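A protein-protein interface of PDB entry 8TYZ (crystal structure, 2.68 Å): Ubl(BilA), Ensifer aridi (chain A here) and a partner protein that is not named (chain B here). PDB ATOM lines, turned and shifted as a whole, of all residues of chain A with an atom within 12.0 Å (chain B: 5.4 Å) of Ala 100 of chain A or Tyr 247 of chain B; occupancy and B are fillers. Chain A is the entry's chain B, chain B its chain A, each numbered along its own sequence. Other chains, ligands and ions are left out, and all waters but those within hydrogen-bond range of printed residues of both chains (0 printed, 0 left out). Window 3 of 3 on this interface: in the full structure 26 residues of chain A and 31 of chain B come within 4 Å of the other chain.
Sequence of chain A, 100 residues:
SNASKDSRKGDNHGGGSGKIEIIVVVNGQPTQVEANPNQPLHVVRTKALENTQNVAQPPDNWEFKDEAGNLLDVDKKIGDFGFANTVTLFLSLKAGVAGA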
ATOM      1  N   GLY A  96      -1.044  25.177   1.606  1.00  0.00           N
ATOM      2  CA  GLY A  96      -0.988  25.471   3.019  1.00  0.00           C
ATOM      3  C   GLY A  96      -0.541  26.882   3.259  1.00  0.00           C
ATOM      4  O   GLY A  96      -0.120  27.577   2.341  1.00  0.00           O
ATOM      5  N   VAL A  97      -0.634  27.312   4.512  1.00  0.00           N
ATOM      6  CA  VAL A  97      -0.149  28.637   4.882  1.00  0.00           C
ATOM      7  C   VAL A  97       0.993  28.603   5.894  1.00  0.00           C
ATOM      8  O   VAL A  97       1.671  29.629   6.050  1.00  0.00           O
ATOM      9  CB  VAL A  97      -1.297  29.534   5.391  1.00  0.00           C
ATOM     10  CG1 VAL A  97      -2.385  29.657   4.348  1.00  0.00           C
ATOM     11  CG2 VAL A  97      -1.851  29.033   6.716  1.00  0.00           C
ATOM     12  N   ALA A  98       1.277  27.473   6.550  1.00  0.00           N
ATOM     13  CA  ALA A  98       2.250  27.443   7.642  1.00  0.00           C
ATOM     14  C   ALA A  98       3.679  27.427   7.111  1.00  0.00           C
ATOM     15  O   ALA A  98       3.985  26.695   6.171  1.00  0.00           O
ATOM     16  CB  ALA A  98       2.029  26.222   8.547  1.00  0.00           C
ATOM     17  N   GLY A  99       4.557  28.225   7.726  1.00  0.00           N
ATOM     18  CA  GLY A  99       5.958  28.294   7.346  1.00  0.00           C
ATOM     19  C   GLY A  99       6.925  28.649   8.462  1.00  0.00           C
ATOM     20  O   GLY A  99       8.115  28.304   8.405  1.00  0.00           O
ATOM     21  N   ALA A 100       6.436  29.353   9.479  1.00  0.00           N
ATOM     22  CA  ALA A 100       7.257  29.720  10.628  1.00  0.00           C
ATOM     23  C   ALA A 100       7.448  28.555  11.570  1.00  0.00           C
ATOM     24  O   ALA A 100       7.931  28.798  12.679  1.00  0.00           O
ATOM     25  CB  ALA A 100       6.628  30.902  11.394  1.00  0.00           C
ATOM     26  OXT ALA A 100       7.101  27.392  11.295  1.00  0.00           O
ATOM     27  N   ARG B  62      15.872  16.728  17.859  1.00  0.00           N
ATOM     28  CA  ARG B  62      14.747  17.563  18.237  1.00  0.00           C
ATOM     29  C   ARG B  62      13.552  16.751  18.680  1.00  0.00           C
ATOM     30  O   ARG B  62      12.450  17.298  18.811  1.00  0.00           O
ATOM     31  CB  ARG B  62      14.365  18.473  17.073  1.00  0.00           C
ATOM     32  CG  ARG B  62      15.509  19.372  16.722  1.00  0.00           C
ATOM     33  CD  ARG B  62      15.273  20.305  15.598  1.00  0.00           C
ATOM     34  NE  ARG B  62      16.559  20.898  15.261  1.00  0.00           N
ATOM     35  CZ  ARG B  62      17.069  21.967  15.855  1.00  0.00           C
ATOM     36  NH1 ARG B  62      16.406  22.614  16.798  1.00  0.00           N
ATOM     37  NH2 ARG B  62      18.268  22.411  15.485  1.00  0.00           N
ATOM     38  N   LEU B 210      11.751  34.072   8.122  1.00  0.00           N
ATOM     39  CA  LEU B 210      12.914  33.258   8.455  1.00  0.00           C
ATOM     40  C   LEU B 210      12.648  32.326   9.628  1.00  0.00           C
ATOM     41  O   LEU B 210      13.352  32.384  10.646  1.00  0.00           O
ATOM     42  CB  LEU B 210      14.116  34.161   8.738  1.00  0.00           C
ATOM     43  CG  LEU B 210      14.530  35.063   7.583  1.00  0.00           C
ATOM     44  CD1 LEU B 210      15.635  35.997   8.012  1.00  0.00           C
ATOM     45  CD2 LEU B 210      14.957  34.237   6.404  1.00  0.00           C
ATOM     46  N   GLY B 211      11.649  31.449   9.470  1.00  0.00           N
ATOM     47  CA  GLY B 211      11.293  30.461  10.475  1.00  0.00           C
ATOM     48  C   GLY B 211      11.666  29.062  10.051  1.00  0.00           C
ATOM     49  O   GLY B 211      12.695  28.880   9.400  1.00  0.00           O
ATOM     50  N   ALA B 212      10.813  28.078  10.357  1.00  0.00           N
ATOM     51  CA  ALA B 212      11.183  26.666  10.207  1.00  0.00           C
ATOM     52  C   ALA B 212      11.519  26.307   8.763  1.00  0.00           C
ATOM     53  O   ALA B 212      12.580  25.721   8.488  1.00  0.00           O
ATOM     54  CB  ALA B 212      10.054  25.777  10.725  1.00  0.00           C
ATOM     55  N   ILE B 213      10.610  26.618   7.828  1.00  0.00           N
ATOM     56  CA  ILE B 213      10.889  26.340   6.419  1.00  0.00           C
ATOM     57  C   ILE B 213      12.173  27.037   5.981  1.00  0.00           C
ATOM     58  O   ILE B 213      13.053  26.419   5.369  1.00  0.00           O
ATOM     59  CB  ILE B 213       9.703  26.744   5.524  1.00  0.00           C
ATOM     60  CG1 ILE B 213       8.528  25.793   5.724  1.00  0.00           C
ATOM     61  CG2 ILE B 213      10.150  26.766   4.077  1.00  0.00           C
ATOM     62  CD1 ILE B 213       7.348  26.069   4.837  1.00  0.00           C
ATOM     63  N   HIS B 215      14.743  27.793   7.498  1.00  0.00           N
ATOM     64  CA  HIS B 215      15.945  27.175   8.051  1.00  0.00           C
ATOM     65  C   HIS B 215      16.415  25.999   7.202  1.00  0.00           C
ATOM     66  O   HIS B 215      17.620  25.780   7.047  1.00  0.00           O
ATOM     67  CB  HIS B 215      15.688  26.703   9.475  1.00  0.00           C
ATOM     68  CG  HIS B 215      16.000  27.719  10.507  1.00  0.00           C
ATOM     69  ND1 HIS B 215      16.735  27.425  11.632  1.00  0.00           N
ATOM     70  CD2 HIS B 215      15.683  29.029  10.586  1.00  0.00           C
ATOM     71  CE1 HIS B 215      16.862  28.518  12.361  1.00  0.00           C
ATOM     72  NE2 HIS B 215      16.231  29.502  11.749  1.00  0.00           N
ATOM     73  N   VAL B 239      14.333  33.975  17.739  1.00  0.00           N
ATOM     74  CA  VAL B 239      14.110  32.557  18.011  1.00  0.00           C
ATOM     75  C   VAL B 239      13.613  32.385  19.438  1.00  0.00           C
ATOM     76  O   VAL B 239      14.146  32.995  20.373  1.00  0.00           O
ATOM     77  CB  VAL B 239      15.402  31.756  17.784  1.00  0.00           C
ATOM     78  CG1 VAL B 239      15.194  30.335  18.224  1.00  0.00           C
ATOM     79  CG2 VAL B 239      15.815  31.800  16.341  1.00  0.00           C
ATOM     80  N   ASN B 243      10.578  27.142  19.293  1.00  0.00           N
ATOM     81  CA  ASN B 243      10.989  27.057  17.894  1.00  0.00           C
ATOM     82  C   ASN B 243      12.059  26.011  17.665  1.00  0.00           C
ATOM     83  O   ASN B 243      12.184  25.515  16.538  1.00  0.00           O
ATOM     84  CB  ASN B 243      11.522  28.398  17.388  1.00  0.00           C
ATOM     85  CG  ASN B 243      10.482  29.473  17.414  1.00  0.00           C
ATOM     86  OD1 ASN B 243       9.287  29.176  17.422  1.00  0.00           O
ATOM     87  ND2 ASN B 243      10.917  30.732  17.439  1.00  0.00           N
ATOM     88  N   LEU B 244      12.835  25.662  18.696  1.00  0.00           N
ATOM     89  CA  LEU B 244      13.897  24.683  18.505  1.00  0.00           C
ATOM     90  C   LEU B 244      13.361  23.297  18.212  1.00  0.00           C
ATOM     91  O   LEU B 244      14.156  22.379  18.008  1.00  0.00           O
ATOM     92  CB  LEU B 244      14.818  24.657  19.721  1.00  0.00           C
ATOM     93  CG  LEU B 244      16.015  25.597  19.751  1.00  0.00           C
ATOM     94  CD1 LEU B 244      15.628  27.081  19.764  1.00  0.00           C
ATOM     95  CD2 LEU B 244      16.872  25.257  20.953  1.00  0.00           C
ATOM     96  N   GLN B 245      12.042  23.139  18.154  1.00  0.00           N
ATOM     97  CA  GLN B 245      11.437  21.883  17.742  1.00  0.00           C
ATOM     98  C   GLN B 245      11.444  21.685  16.218  1.00  0.00           C
ATOM     99  O   GLN B 245      11.415  20.531  15.764  1.00  0.00           O
ATOM    100  CB  GLN B 245      10.028  21.820  18.344  1.00  0.00           C
ATOM    101  CG  GLN B 245       9.144  20.678  17.901  1.00  0.00           C
ATOM    102  CD  GLN B 245       8.330  21.013  16.671  1.00  0.00           C
ATOM    103  OE1 GLN B 245       7.988  22.170  16.452  1.00  0.00           O
ATOM    104  NE2 GLN B 245       8.027  20.000  15.854  1.00  0.00           N
ATOM    105  N   ARG B 246      11.514  22.762  15.415  1.00  0.00           N
ATOM    106  CA  ARG B 246      11.643  22.625  13.958  1.00  0.00           C
ATOM    107  C   ARG B 246      12.809  23.372  13.345  1.00  0.00           C
ATOM    108  O   ARG B 246      13.148  23.080  12.190  1.00  0.00           O
ATOM    109  CB  ARG B 246      10.418  23.148  13.190  1.00  0.00           C
ATOM    110  CG  ARG B 246       9.066  23.071  13.788  1.00  0.00           C
ATOM    111  CD  ARG B 246       8.265  24.280  13.344  1.00  0.00           C
ATOM    112  NE  ARG B 246       7.887  25.008  14.537  1.00  0.00           N
ATOM    113  CZ  ARG B 246       7.044  26.018  14.556  1.00  0.00           C
ATOM    114  NH1 ARG B 246       6.470  26.452  13.449  1.00  0.00           N
ATOM    115  NH2 ARG B 246       6.745  26.581  15.716  1.00  0.00           N
ATOM    116  N   TYR B 247      13.347  24.396  13.997  1.00  0.00           N
ATOM    117  CA  TYR B 247      14.345  25.265  13.362  1.00  0.00           C
ATOM    118  C   TYR B 247      15.670  24.505  13.345  1.00  0.00           C
ATOM    119  O   TYR B 247      16.376  24.454  14.350  1.00  0.00           O
ATOM    120  CB  TYR B 247      14.484  26.590  14.109  1.00  0.00           C
ATOM    121  CG  TYR B 247      13.348  27.589  14.012  1.00  0.00           C
ATOM    122  CD1 TYR B 247      12.033  27.191  13.822  1.00  0.00           C
ATOM    123  CD2 TYR B 247      13.600  28.955  14.107  1.00  0.00           C
ATOM    124  CE1 TYR B 247      11.005  28.117  13.739  1.00  0.00           C
ATOM    125  CE2 TYR B 247      12.564  29.893  14.022  1.00  0.00           C
ATOM    126  CZ  TYR B 247      11.277  29.466  13.835  1.00  0.00           C
ATOM    127  OH  TYR B 247      10.240  30.364  13.748  1.00  0.00           O
ATOM    128  N   VAL B 248      16.020  23.895  12.212  1.00  0.00           N
ATOM    129  CA  VAL B 248      17.169  23.004  12.207  1.00  0.00           C
ATOM    130  C   VAL B 248      18.482  23.731  12.420  1.00  0.00           C
ATOM    131  O   VAL B 248      19.501  23.087  12.673  1.00  0.00           O
ATOM    132  CB  VAL B 248      17.241  22.181  10.907  1.00  0.00           C
ATOM    133  CG1 VAL B 248      16.029  21.264  10.799  1.00  0.00           C
ATOM    134  CG2 VAL B 248      17.370  23.075   9.688  1.00  0.00           C
ATOM    135  N   LEU B 249      18.498  25.057  12.343  1.00  0.00           N
ATOM    136  CA  LEU B 249      19.728  25.813  12.554  1.00  0.00           C
ATOM    137  C   LEU B 249      19.732  26.587  13.864  1.00  0.00           C
ATOM    138  O   LEU B 249      20.574  27.484  14.037  1.00  0.00           O
ATOM    139  CB  LEU B 249      19.979  26.778  11.393  1.00  0.00           C
ATOM    140  CG  LEU B 249      20.206  26.095  10.063  1.00  0.00           C
ATOM    141  CD1 LEU B 249      20.708  27.124   9.118  1.00  0.00           C
ATOM    142  CD2 LEU B 249      21.190  24.970  10.242  1.00  0.00           C
ATOM    143  N   ALA B 250      18.832  26.260  14.789  1.00  0.00           N
ATOM    144  CA  ALA B 250      18.734  26.940  16.069  1.00  0.00           C
ATOM    145  C   ALA B 250      18.955  25.918  17.176  1.00  0.00           C
ATOM    146  O   ALA B 250      18.095  25.067  17.417  1.00  0.00           O
ATOM    147  CB  ALA B 250      17.383  27.636  16.206  1.00  0.00           C
ATOM    148  N   GLY B 251      20.119  25.977  17.825  1.00  0.00           N
ATOM    149  CA  GLY B 251      20.350  25.284  19.076  1.00  0.00           C
ATOM    150  C   GLY B 251      19.988  26.160  20.265  1.00  0.00           C
ATOM    151  O   GLY B 251      19.406  27.239  20.127  1.00  0.00           O
ATOM    152  N   LYS B 259      16.078  36.296  14.160  1.00  0.00           N
ATOM    153  CA  LYS B 259      16.057  35.345  13.050  1.00  0.00           C
ATOM    154  C   LYS B 259      16.837  35.882  11.854  1.00  0.00           C
ATOM    155  O   LYS B 259      17.530  35.130  11.158  1.00  0.00           O
ATOM    156  CB  LYS B 259      14.621  35.020  12.649  1.00  0.00           C
ATOM    157  CG  LYS B 259      13.783  34.364  13.723  1.00  0.00           C
ATOM    158  CD  LYS B 259      12.417  34.052  13.169  1.00  0.00           C
ATOM    159  CE  LYS B 259      11.449  33.490  14.198  1.00  0.00           C
ATOM    160  NZ  LYS B 259      10.109  33.431  13.558  1.00  0.00           N
ATOM    161  N   ALA B 299       8.407  32.097   2.602  1.00  0.00           N
ATOM    162  CA  ALA B 299       8.203  31.097   3.641  1.00  0.00           C
ATOM    163  C   ALA B 299       7.566  31.761   4.862  1.00  0.00           C
ATOM    164  O   ALA B 299       8.066  31.686   5.987  1.00  0.00           O
ATOM    165  CB  ALA B 299       9.519  30.411   3.984  1.00  0.00           C
ATOM    166  N   LEU B 300       6.457  32.454   4.622  1.00  0.00           N
ATOM    167  CA  LEU B 300       5.711  33.180   5.635  1.00  0.00           C
ATOM    168  C   LEU B 300       4.705  32.236   6.299  1.00  0.00           C
ATOM    169  O   LEU B 300       4.801  31.010   6.178  1.00  0.00           O
ATOM    170  CB  LEU B 300       5.062  34.393   4.995  1.00  0.00           C
ATOM    171  CG  LEU B 300       6.052  35.393   4.374  1.00  0.00           C
ATOM    172  CD1 LEU B 300       5.340  36.407   3.475  1.00  0.00           C
ATOM    173  CD2 LEU B 300       6.830  36.110   5.466  1.00  0.00           C
ATOM    174  N   ASP B 301       3.726  32.791   7.019  1.00  0.00           N
ATOM    175  CA  ASP B 301       2.897  31.975   7.906  1.00  0.00           C
ATOM    176  C   ASP B 301       1.398  32.159   7.737  1.00  0.00           C
ATOM    177  O   ASP B 301       0.631  31.446   8.393  1.00  0.00           O
ATOM    178  CB  ASP B 301       3.243  32.246   9.376  1.00  0.00           C
ATOM    179  CG  ASP B 301       3.368  30.986  10.180  1.00  0.00           C
ATOM    180  OD1 ASP B 301       3.677  29.943   9.574  1.00  0.00           O
ATOM    181  OD2 ASP B 301       3.145  31.039  11.413  1.00  0.00           O
ATOM    182  N   PRO B 436       4.132  21.897  12.616  1.00  0.00           N
ATOM    183  CA  PRO B 436       4.616  20.807  11.777  1.00  0.00           C
ATOM    184  C   PRO B 436       5.797  20.061  12.384  1.00  0.00           C
ATOM    185  O   PRO B 436       6.486  20.548  13.293  1.00  0.00           O
ATOM    186  CB  PRO B 436       5.042  21.538  10.497  1.00  0.00           C
ATOM    187  CG  PRO B 436       5.553  22.793  11.010  1.00  0.00           C
ATOM    188  CD  PRO B 436       4.640  23.200  12.143  1.00  0.00           C
ATOM    189  N   SER B 441       9.279  20.728   7.835  1.00  0.00           N
ATOM    190  CA  SER B 441       9.843  22.059   7.672  1.00  0.00           C
ATOM    191  C   SER B 441      11.189  22.016   6.957  1.00  0.00           C
ATOM    192  O   SER B 441      11.443  22.793   6.024  1.00  0.00           O
ATOM    193  CB  SER B 441       9.972  22.713   9.042  1.00  0.00           C
ATOM    194  OG  SER B 441       8.686  23.030   9.571  1.00  0.00           O
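Gly 96 of chain A touches none of the printed residues of chain B.
Of the printed residues of chain B, Ala 98 of chain A touches Ile 213 (3.7 Å), Leu 300 (3.9 Å) and Asp 301 (3.5 Å).
Of the printed residues of chain B, Gly 99 of chain A touches Gly 211 (3.99 Å), Ala 212 (3.3 Å), Ile 213 (3.1 Å), Leu 300 (3.2 Å) and Asp 301 (2.7 Å).
Ala 100 of chain A touches four residues of chain B.
Of the printed residues of chain A, Gly 211 of chain B touches Gly 99 (3.99 Å).
Ala 212 of chain B touches just these residues of chain A: Gly 99 (3.3 Å) and Ala 100 (3.4 Å).
Of the printed residues of chain A, Ile 213 of chain B touches Ala 98 and Gly 99.
No residue of chain A comes within 4 Å of His 215 of chain B.
Val 239 of chain B touches none of the printed residues of chain A.
No residue of chain A comes within 4 Å of Asn 243 of chain B.
No residue of chain A comes within 4 Å of Leu 244 of chain B.
Gln 245 of chain B touches none of the printed residues of chain A.
Of chain A, only Ala 100 comes within 4 Å of Arg 246 of chain B.
Tyr 247 of chain B touches just one residue of chain A: Ala 100 (3.0 Å).
No residue of chain A comes within 4 Å of Val 248 of chain B.
Leu 249 of chain B touches none of the printed residues of chain A.
No residue of chain A comes within 4 Å of Ala 250 of chain B.
Asp 301 of chain B touches four residues of chain A.
Pro 436 of chain B touches none of the printed residues of chain A.
The nearest residue of chain A that does not touch Tyr 247 of chain B is Gly 99 of chain A (6.1 Å).
The backbone carbonyl oxygen of Tyr 247 of chain B sits close to the guanidinium group of Arg 62 of chain B (3.0 Å).
The side-chain amide oxygen (OE1) of Gln 245 of chain B lies close to the guanidinium group (NE) of Arg 246 of chain B (3.4 Å).
OH of Tyr 247 of chain B sits at hydrogen-bond distance from NZ of Lys 259 of chain B, 3.1 Å away.
The guanidinium group (NH1) of Arg 246 of chain B lies within salt-bridge range of the chain-end carboxylate (OXT) of Ala 100 of chain A, 2.4 Å away.
The backbone NH (N) of Gly 99 of chain A sits at hydrogen-bond distance from the side-chain carboxylate (OD1) of Asp 301 of chain B (2.7 Å).
The backbone carbonyl oxygen (O) of Val 97 of chain A lies close to the backbone carbonyl oxygen (O) of Asp 301 of chain B, 3.1 Å away.
O of Gly 99 of chain A lies within hydrogen-bond range of N of Ile 213 of chain B (3.1 Å).
OH of Tyr 247 of chain B lies within hydrogen-bond range of O of Ala 100 of chain A (3.0 Å).
The backbone NH of Ala 100 of chain A is in hydrogen-bond range of the side-chain carboxylate of Asp 301 of chain B, 2.8 Å away.
The backbone carbonyl oxygen of Leu 300 of chain B lies close to the backbone NH of Gly 99 of chain A, 3.2 Å away.
O of Val 97 of chain A lies close to O of Leu 300 of chain B.
The backbone NH (N) of Ala 212 of chain B is in hydrogen-bond range of the backbone carbonyl oxygen (O) of Gly 99 of chain A (3.3 Å).
O of Ala 98 of chain A touches CD1 of Ile 213 of chain B, 3.7 Å away.
C of Ala 98 of chain A touches O of Leu 300 of chain B (3.9 Å).
Ala 98 of chain A touches Asp 301 of chain B (CA to OD1, 3.5 Å).
O of Gly 99 of chain A touches C of Gly 211 of chain B, 3.99 Å away.
Ala 212 of chain B touches Ala 100 of chain A.
Of the 5 printed residues of chain A, 4 touch a printed residue of chain B.
Hydrophobic or aromatic side chains of chain A that line the printed part of chain B: Val 97 and Ala 100.
Along chain B the printed residues that touch a printed residue of chain A span positions 211 to 301.
Among the printed residues, 14 pairs touch across the chains.
Among the printed residues, no Asp or Glu carboxylate lies within 4 Å of a Lys or Arg side-chain nitrogen of the other chain.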
